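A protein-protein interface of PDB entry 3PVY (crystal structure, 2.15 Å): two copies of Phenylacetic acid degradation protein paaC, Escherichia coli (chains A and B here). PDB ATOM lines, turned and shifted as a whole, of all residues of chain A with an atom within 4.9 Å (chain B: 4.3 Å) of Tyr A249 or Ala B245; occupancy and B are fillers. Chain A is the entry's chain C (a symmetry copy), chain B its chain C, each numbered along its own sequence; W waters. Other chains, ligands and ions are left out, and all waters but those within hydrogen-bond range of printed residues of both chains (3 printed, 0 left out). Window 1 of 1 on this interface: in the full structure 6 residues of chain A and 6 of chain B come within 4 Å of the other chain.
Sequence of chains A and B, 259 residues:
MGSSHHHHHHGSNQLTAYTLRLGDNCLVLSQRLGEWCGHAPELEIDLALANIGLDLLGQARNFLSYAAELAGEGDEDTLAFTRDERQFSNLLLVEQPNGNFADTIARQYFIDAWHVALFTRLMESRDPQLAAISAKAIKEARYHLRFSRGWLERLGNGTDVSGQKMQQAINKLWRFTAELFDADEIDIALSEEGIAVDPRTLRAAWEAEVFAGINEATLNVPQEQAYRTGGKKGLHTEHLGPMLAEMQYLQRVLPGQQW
The side-chain amide oxygen (OE1) of Gln B248 lies within hydrogen-bond range of the side-chain hydroxyl (OH) of Tyr A249 (2.7 Å).
OH of Tyr B249 sits at hydrogen-bond distance from OE1 of Gln A248.
OE1 of Gln B248 is in hydrogen-bond range of NH2 of Arg B252, 2.9 Å away.
The side-chain amide oxygen (OE1) of Gln A248 sits at hydrogen-bond distance from the guanidinium group (NH2) of Arg A252, at 2.9 Å.
Among the printed residues, merely in contact across the chains: Leu A244 with Tyr B249 (3.9 Å), Ala A245 with Tyr B249 (3.6 Å), Tyr A249 with Leu B244 (3.9 Å), Tyr A249 with Ala B245 (3.6 Å), Tyr A249 with Arg B252 (3.8 Å), Arg A252 with Tyr B249 (3.8 Å), Arg A252 with Arg B252 (3.6 Å) and Val A253 with Arg B252 (3.7 Å).
Of chain B, only Leu B244, Ala B245, Gln B248 and Arg B252 come within 4 Å of Tyr A249.
Of the printed residues of chain B, Arg A252 touches Tyr B249 and Arg B252.
Of the printed residues of chain A, Gln B248 touches Tyr A249 (2.7 Å).
Printed residues of chain A within 4 Å of Tyr B249: Leu A244 (3.9 Å), Ala A245 (3.6 Å), Gln A248 (2.7 Å) and Arg A252 (3.8 Å).
Of the printed residues of chain A, Arg B252 touches Tyr A249, Arg A252 and Val A253.
Of the printed residues of chain B, Gln A248 touches Tyr B249.
Glu B246 touches none of the printed residues of chain A.
Leu A250 touches none of the printed residues of chain B.
The nearest printed residue of chain B that does not touch Tyr A249 is Gly B241 (4.6 Å).
The nearest printed residue of chain B that does not touch Val A253 is Gln B248 (5.3 Å).
Of the 10 printed residues of chain A, 6 touch a printed residue of chain B.
Printed residues of chain A that touch a printed residue of chain B: Leu A244, Ala A245, Gln A248, Tyr A249, Arg A252 and Val A253.
Hydrophobic or aromatic side chains of chain A within 4 Å of the printed part of chain B: Leu A244, Ala A245, Tyr A249 and Val A253.
Along chain A the printed residues that touch a printed residue of chain B span positions 244 to 253.
Among the printed residues, 10 pairs touch across the chains.
Leu A244 touches Tyr B249, and with the chains exchanged Tyr A249 touches Leu B244.
Gln A248 touches Tyr B249, and with the chains exchanged Tyr A249 touches Gln B248.
Tyr A249 touches Arg B252, and with the chains exchanged Arg A252 touches Tyr B249.
Arg B252 touches its own counterpart, Arg A252.
7 positions are printed for both chains.
Of the 10 pairs that touch across the chains among the printed residues, 9 have their exchanged pair printed and touching as well.
Water W3 lies within hydrogen-bond range of O of Ala B245 and O of Ala A245.
Water W1 lies within hydrogen-bond range of the backbone carbonyl oxygen (O) of Arg A252 and the backbone carbonyl oxygen (O) of Arg B252.
Water W2 lies within hydrogen-bond range of the backbone carbonyl oxygen of Arg B252 (2.8 Å) and the backbone carbonyl oxygen of Arg A252 (2.9 Å).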
ATOM      1  N   LEU A 244       3.920  21.716  24.507  1.00  0.00           N
ATOM      2  CA  LEU A 244       3.232  21.299  23.287  1.00  0.00           C
ATOM      3  C   LEU A 244       2.280  22.371  22.798  1.00  0.00           C
ATOM      4  O   LEU A 244       2.097  22.545  21.586  1.00  0.00           O
ATOM      5  CB  LEU A 244       2.479  19.988  23.507  1.00  0.00           C
ATOM      6  CG  LEU A 244       3.308  18.744  23.849  1.00  0.00           C
ATOM      7  CD1 LEU A 244       2.415  17.526  23.981  1.00  0.00           C
ATOM      8  CD2 LEU A 244       4.351  18.505  22.787  1.00  0.00           C
ATOM      9  N   ALA A 245       1.681  23.101  23.735  1.00  0.00           N
ATOM     10  CA  ALA A 245       0.821  24.219  23.351  1.00  0.00           C
ATOM     11  C   ALA A 245       1.612  25.162  22.450  1.00  0.00           C
ATOM     12  O   ALA A 245       1.150  25.536  21.374  1.00  0.00           O
ATOM     13  CB  ALA A 245       0.260  24.929  24.568  1.00  0.00           C
ATOM     14  N   GLU A 246       2.824  25.496  22.879  1.00  0.00           N
ATOM     15  CA  GLU A 246       3.696  26.425  22.169  1.00  0.00           C
ATOM     16  C   GLU A 246       4.186  25.772  20.878  1.00  0.00           C
ATOM     17  O   GLU A 246       4.086  26.345  19.795  1.00  0.00           O
ATOM     18  CB  GLU A 246       4.889  26.808  23.088  1.00  0.00           C
ATOM     19  CG  GLU A 246       5.975  27.659  22.421  1.00  0.00           C
ATOM     20  CD  GLU A 246       7.198  27.935  23.339  1.00  0.00           C
ATOM     21  OE1 GLU A 246       7.428  27.189  24.311  1.00  0.00           O
ATOM     22  OE2 GLU A 246       7.947  28.890  23.065  1.00  0.00           O
ATOM     23  N   MET A 247       4.712  24.555  21.003  1.00  0.00           N
ATOM     24  CA  MET A 247       5.264  23.856  19.860  1.00  0.00           C
ATOM     25  C   MET A 247       4.245  23.643  18.746  1.00  0.00           C
ATOM     26  O   MET A 247       4.582  23.807  17.573  1.00  0.00           O
ATOM     27  CB  MET A 247       5.897  22.520  20.279  1.00  0.00           C
ATOM     28  CG  MET A 247       6.560  21.780  19.102  1.00  0.00           C
ATOM     29  SD  MET A 247       7.395  20.247  19.591  1.00  0.00           S
ATOM     30  CE  MET A 247       6.014  19.106  19.630  1.00  0.00           C
ATOM     31  N   GLN A 248       3.006  23.292  19.107  1.00  0.00           N
ATOM     32  CA  GLN A 248       2.025  22.866  18.103  1.00  0.00           C
ATOM     33  C   GLN A 248       1.042  23.938  17.610  1.00  0.00           C
ATOM     34  O   GLN A 248       0.270  23.679  16.680  1.00  0.00           O
ATOM     35  CB  GLN A 248       1.220  21.659  18.612  1.00  0.00           C
ATOM     36  CG  GLN A 248       2.059  20.474  19.044  1.00  0.00           C
ATOM     37  CD  GLN A 248       1.207  19.344  19.562  1.00  0.00           C
ATOM     38  OE1 GLN A 248       0.061  19.551  19.954  1.00  0.00           O
ATOM     39  NE2 GLN A 248       1.758  18.139  19.562  1.00  0.00           N
ATOM     40  N   TYR A 249       1.067  25.120  18.220  1.00  0.00           N
ATOM     41  CA  TYR A 249       0.044  26.148  17.958  1.00  0.00           C
ATOM     42  C   TYR A 249      -0.303  26.312  16.478  1.00  0.00           C
ATOM     43  O   TYR A 249      -1.450  26.132  16.093  1.00  0.00           O
ATOM     44  CB  TYR A 249       0.484  27.497  18.526  1.00  0.00           C
ATOM     45  CG  TYR A 249      -0.522  28.622  18.405  1.00  0.00           C
ATOM     46  CD1 TYR A 249      -1.851  28.465  18.807  1.00  0.00           C
ATOM     47  CD2 TYR A 249      -0.129  29.873  17.905  1.00  0.00           C
ATOM     48  CE1 TYR A 249      -2.771  29.529  18.707  1.00  0.00           C
ATOM     49  CE2 TYR A 249      -1.032  30.933  17.804  1.00  0.00           C
ATOM     50  CZ  TYR A 249      -2.344  30.762  18.209  1.00  0.00           C
ATOM     51  OH  TYR A 249      -3.218  31.832  18.115  1.00  0.00           O
ATOM     52  N   LEU A 250       0.689  26.636  15.659  1.00  0.00           N
ATOM     53  CA  LEU A 250       0.455  26.923  14.239  1.00  0.00           C
ATOM     54  C   LEU A 250      -0.167  25.743  13.489  1.00  0.00           C
ATOM     55  O   LEU A 250      -1.109  25.907  12.698  1.00  0.00           O
ATOM     56  CB  LEU A 250       1.748  27.395  13.556  1.00  0.00           C
ATOM     57  CG  LEU A 250       1.647  27.822  12.085  1.00  0.00           C
ATOM     58  CD1 LEU A 250       0.484  28.811  11.881  1.00  0.00           C
ATOM     59  CD2 LEU A 250       2.947  28.459  11.658  1.00  0.00           C
ATOM     60  N   GLN A 251       0.362  24.554  13.737  1.00  0.00           N
ATOM     61  CA  GLN A 251      -0.156  23.345  13.114  1.00  0.00           C
ATOM     62  C   GLN A 251      -1.597  23.087  13.513  1.00  0.00           C
ATOM     63  O   GLN A 251      -2.402  22.667  12.679  1.00  0.00           O
ATOM     64  CB  GLN A 251       0.733  22.141  13.446  1.00  0.00           C
ATOM     65  CG  GLN A 251       1.956  22.021  12.523  1.00  0.00           C
ATOM     66  CD  GLN A 251       1.631  21.403  11.162  1.00  0.00           C
ATOM     67  OE1 GLN A 251       0.484  21.090  10.874  1.00  0.00           O
ATOM     68  NE2 GLN A 251       2.655  21.230  10.320  1.00  0.00           N
ATOM     69  N   ARG A 252      -1.924  23.364  14.776  1.00  0.00           N
ATOM     70  CA  ARG A 252      -3.301  23.227  15.263  1.00  0.00           C
ATOM     71  C   ARG A 252      -4.245  24.259  14.644  1.00  0.00           C
ATOM     72  O   ARG A 252      -5.400  23.945  14.347  1.00  0.00           O
ATOM     73  CB  ARG A 252      -3.361  23.324  16.793  1.00  0.00           C
ATOM     74  CG  ARG A 252      -2.531  22.284  17.554  1.00  0.00           C
ATOM     75  CD  ARG A 252      -2.815  20.850  17.108  1.00  0.00           C
ATOM     76  NE  ARG A 252      -2.278  19.884  18.072  1.00  0.00           N
ATOM     77  CZ  ARG A 252      -2.756  18.652  18.253  1.00  0.00           C
ATOM     78  NH1 ARG A 252      -3.774  18.208  17.530  1.00  0.00           N
ATOM     79  NH2 ARG A 252      -2.211  17.855  19.164  1.00  0.00           N
ATOM     80  N   VAL A 253      -3.760  25.485  14.465  1.00  0.00           N
ATOM     81  CA  VAL A 253      -4.562  26.550  13.837  1.00  0.00           C
ATOM     82  C   VAL A 253      -4.778  26.283  12.353  1.00  0.00           C
ATOM     83  O   VAL A 253      -5.872  26.488  11.838  1.00  0.00           O
ATOM     84  CB  VAL A 253      -3.915  27.942  13.998  1.00  0.00           C
ATOM     85  CG1 VAL A 253      -4.765  29.025  13.311  1.00  0.00           C
ATOM     86  CG2 VAL A 253      -3.718  28.281  15.478  1.00  0.00           C
ATOM     87  N   GLY B 241       1.974  36.515  21.031  1.00  0.00           N
ATOM     88  CA  GLY B 241       1.890  35.218  20.352  1.00  0.00           C
ATOM     89  C   GLY B 241       1.953  34.003  21.274  1.00  0.00           C
ATOM     90  O   GLY B 241       1.088  33.137  21.215  1.00  0.00           O
ATOM     91  N   PRO B 242       2.998  33.917  22.115  1.00  0.00           N
ATOM     92  CA  PRO B 242       3.111  32.818  23.085  1.00  0.00           C
ATOM     93  C   PRO B 242       1.950  32.758  24.095  1.00  0.00           C
ATOM     94  O   PRO B 242       1.536  31.659  24.473  1.00  0.00           O
ATOM     95  CB  PRO B 242       4.444  33.108  23.782  1.00  0.00           C
ATOM     96  CG  PRO B 242       5.267  33.781  22.674  1.00  0.00           C
ATOM     97  CD  PRO B 242       4.261  34.672  21.987  1.00  0.00           C
ATOM     98  N   MET B 243       1.422  33.915  24.495  1.00  0.00           N
ATOM     99  CA  MET B 243       0.219  33.970  25.344  1.00  0.00           C
ATOM    100  C   MET B 243      -0.984  33.270  24.693  1.00  0.00           C
ATOM    101  O   MET B 243      -1.664  32.464  25.333  1.00  0.00           O
ATOM    102  CB  MET B 243      -0.149  35.418  25.647  1.00  0.00           C
ATOM    103  CG  MET B 243       0.716  36.088  26.705  1.00  0.00           C
ATOM    104  SD  MET B 243       0.010  37.679  27.253  1.00  0.00           S
ATOM    105  CE  MET B 243      -1.347  37.093  28.253  1.00  0.00           C
ATOM    106  N   LEU B 244      -1.229  33.571  23.413  1.00  0.00           N
ATOM    107  CA  LEU B 244      -2.376  33.013  22.701  1.00  0.00           C
ATOM    108  C   LEU B 244      -2.175  31.541  22.400  1.00  0.00           C
ATOM    109  O   LEU B 244      -3.135  30.760  22.408  1.00  0.00           O
ATOM    110  CB  LEU B 244      -2.642  33.782  21.408  1.00  0.00           C
ATOM    111  CG  LEU B 244      -3.029  35.261  21.531  1.00  0.00           C
ATOM    112  CD1 LEU B 244      -3.308  35.855  20.165  1.00  0.00           C
ATOM    113  CD2 LEU B 244      -4.242  35.410  22.415  1.00  0.00           C
ATOM    114  N   ALA B 245      -0.927  31.156  22.145  1.00  0.00           N
ATOM    115  CA  ALA B 245      -0.628  29.740  21.939  1.00  0.00           C
ATOM    116  C   ALA B 245      -1.131  28.950  23.143  1.00  0.00           C
ATOM    117  O   ALA B 245      -1.837  27.956  22.990  1.00  0.00           O
ATOM    118  CB  ALA B 245       0.851  29.519  21.689  1.00  0.00           C
ATOM    119  N   GLU B 246      -0.803  29.435  24.336  1.00  0.00           N
ATOM    120  CA  GLU B 246      -1.158  28.780  25.590  1.00  0.00           C
ATOM    121  C   GLU B 246      -2.666  28.893  25.811  1.00  0.00           C
ATOM    122  O   GLU B 246      -3.348  27.904  26.070  1.00  0.00           O
ATOM    123  CB  GLU B 246      -0.373  29.449  26.753  1.00  0.00           C
ATOM    124  CG  GLU B 246      -0.761  28.970  28.157  1.00  0.00           C
ATOM    125  CD  GLU B 246      -0.029  29.732  29.296  1.00  0.00           C
ATOM    126  OE1 GLU B 246       0.458  30.859  29.079  1.00  0.00           O
ATOM    127  OE2 GLU B 246       0.031  29.208  30.423  1.00  0.00           O
ATOM    128  N   MET B 247      -3.183  30.114  25.695  1.00  0.00           N
ATOM    129  CA  MET B 247      -4.590  30.359  25.937  1.00  0.00           C
ATOM    130  C   MET B 247      -5.500  29.547  25.020  1.00  0.00           C
ATOM    131  O   MET B 247      -6.514  29.023  25.479  1.00  0.00           O
ATOM    132  CB  MET B 247      -4.919  31.857  25.839  1.00  0.00           C
ATOM    133  CG  MET B 247      -6.392  32.166  26.162  1.00  0.00           C
ATOM    134  SD  MET B 247      -6.780  33.937  26.144  1.00  0.00           S
ATOM    135  CE  MET B 247      -7.027  34.212  24.390  1.00  0.00           C
ATOM    136  N   GLN B 248      -5.134  29.433  23.739  1.00  0.00           N
ATOM    137  CA  GLN B 248      -6.048  28.853  22.749  1.00  0.00           C
ATOM    138  C   GLN B 248      -5.844  27.366  22.420  1.00  0.00           C
ATOM    139  O   GLN B 248      -6.653  26.785  21.687  1.00  0.00           O
ATOM    140  CB  GLN B 248      -6.004  29.655  21.437  1.00  0.00           C
ATOM    141  CG  GLN B 248      -6.288  31.135  21.591  1.00  0.00           C
ATOM    142  CD  GLN B 248      -6.195  31.862  20.274  1.00  0.00           C
ATOM    143  OE1 GLN B 248      -5.570  31.378  19.333  1.00  0.00           O
ATOM    144  NE2 GLN B 248      -6.820  33.027  20.195  1.00  0.00           N
ATOM    145  N   TYR B 249      -4.786  26.760  22.951  1.00  0.00           N
ATOM    146  CA  TYR B 249      -4.393  25.397  22.551  1.00  0.00           C
ATOM    147  C   TYR B 249      -5.566  24.426  22.430  1.00  0.00           C
ATOM    148  O   TYR B 249      -5.798  23.872  21.363  1.00  0.00           O
ATOM    149  CB  TYR B 249      -3.364  24.829  23.528  1.00  0.00           C
ATOM    150  CG  TYR B 249      -2.806  23.465  23.178  1.00  0.00           C
ATOM    151  CD1 TYR B 249      -2.305  23.183  21.905  1.00  0.00           C
ATOM    152  CD2 TYR B 249      -2.755  22.451  24.145  1.00  0.00           C
ATOM    153  CE1 TYR B 249      -1.770  21.914  21.599  1.00  0.00           C
ATOM    154  CE2 TYR B 249      -2.225  21.192  23.854  1.00  0.00           C
ATOM    155  CZ  TYR B 249      -1.730  20.930  22.589  1.00  0.00           C
ATOM    156  OH  TYR B 249      -1.194  19.680  22.327  1.00  0.00           O
ATOM    157  N   ARG B 252      -8.111  25.159  19.746  1.00  0.00           N
ATOM    158  CA  ARG B 252      -7.518  24.880  18.434  1.00  0.00           C
ATOM    159  C   ARG B 252      -7.450  23.382  18.130  1.00  0.00           C
ATOM    160  O   ARG B 252      -7.662  22.969  16.988  1.00  0.00           O
ATOM    161  CB  ARG B 252      -6.117  25.495  18.315  1.00  0.00           C
ATOM    162  CG  ARG B 252      -6.045  27.014  18.504  1.00  0.00           C
ATOM    163  CD  ARG B 252      -7.029  27.775  17.615  1.00  0.00           C
ATOM    164  NE  ARG B 252      -6.698  29.202  17.565  1.00  0.00           N
ATOM    165  CZ  ARG B 252      -7.008  30.016  16.555  1.00  0.00           C
ATOM    166  NH1 ARG B 252      -7.675  29.564  15.502  1.00  0.00           N
ATOM    167  NH2 ARG B 252      -6.649  31.293  16.596  1.00  0.00           N
HETATM  168  O   HOH W   1      -6.306  21.401  14.970  1.00  0.00           O
HETATM  169  O   HOH W   2      -8.097  24.801  14.954  1.00  0.00           O
HETATM  170  O   HOH W   3      -1.375  26.200  21.097  1.00  0.00           O
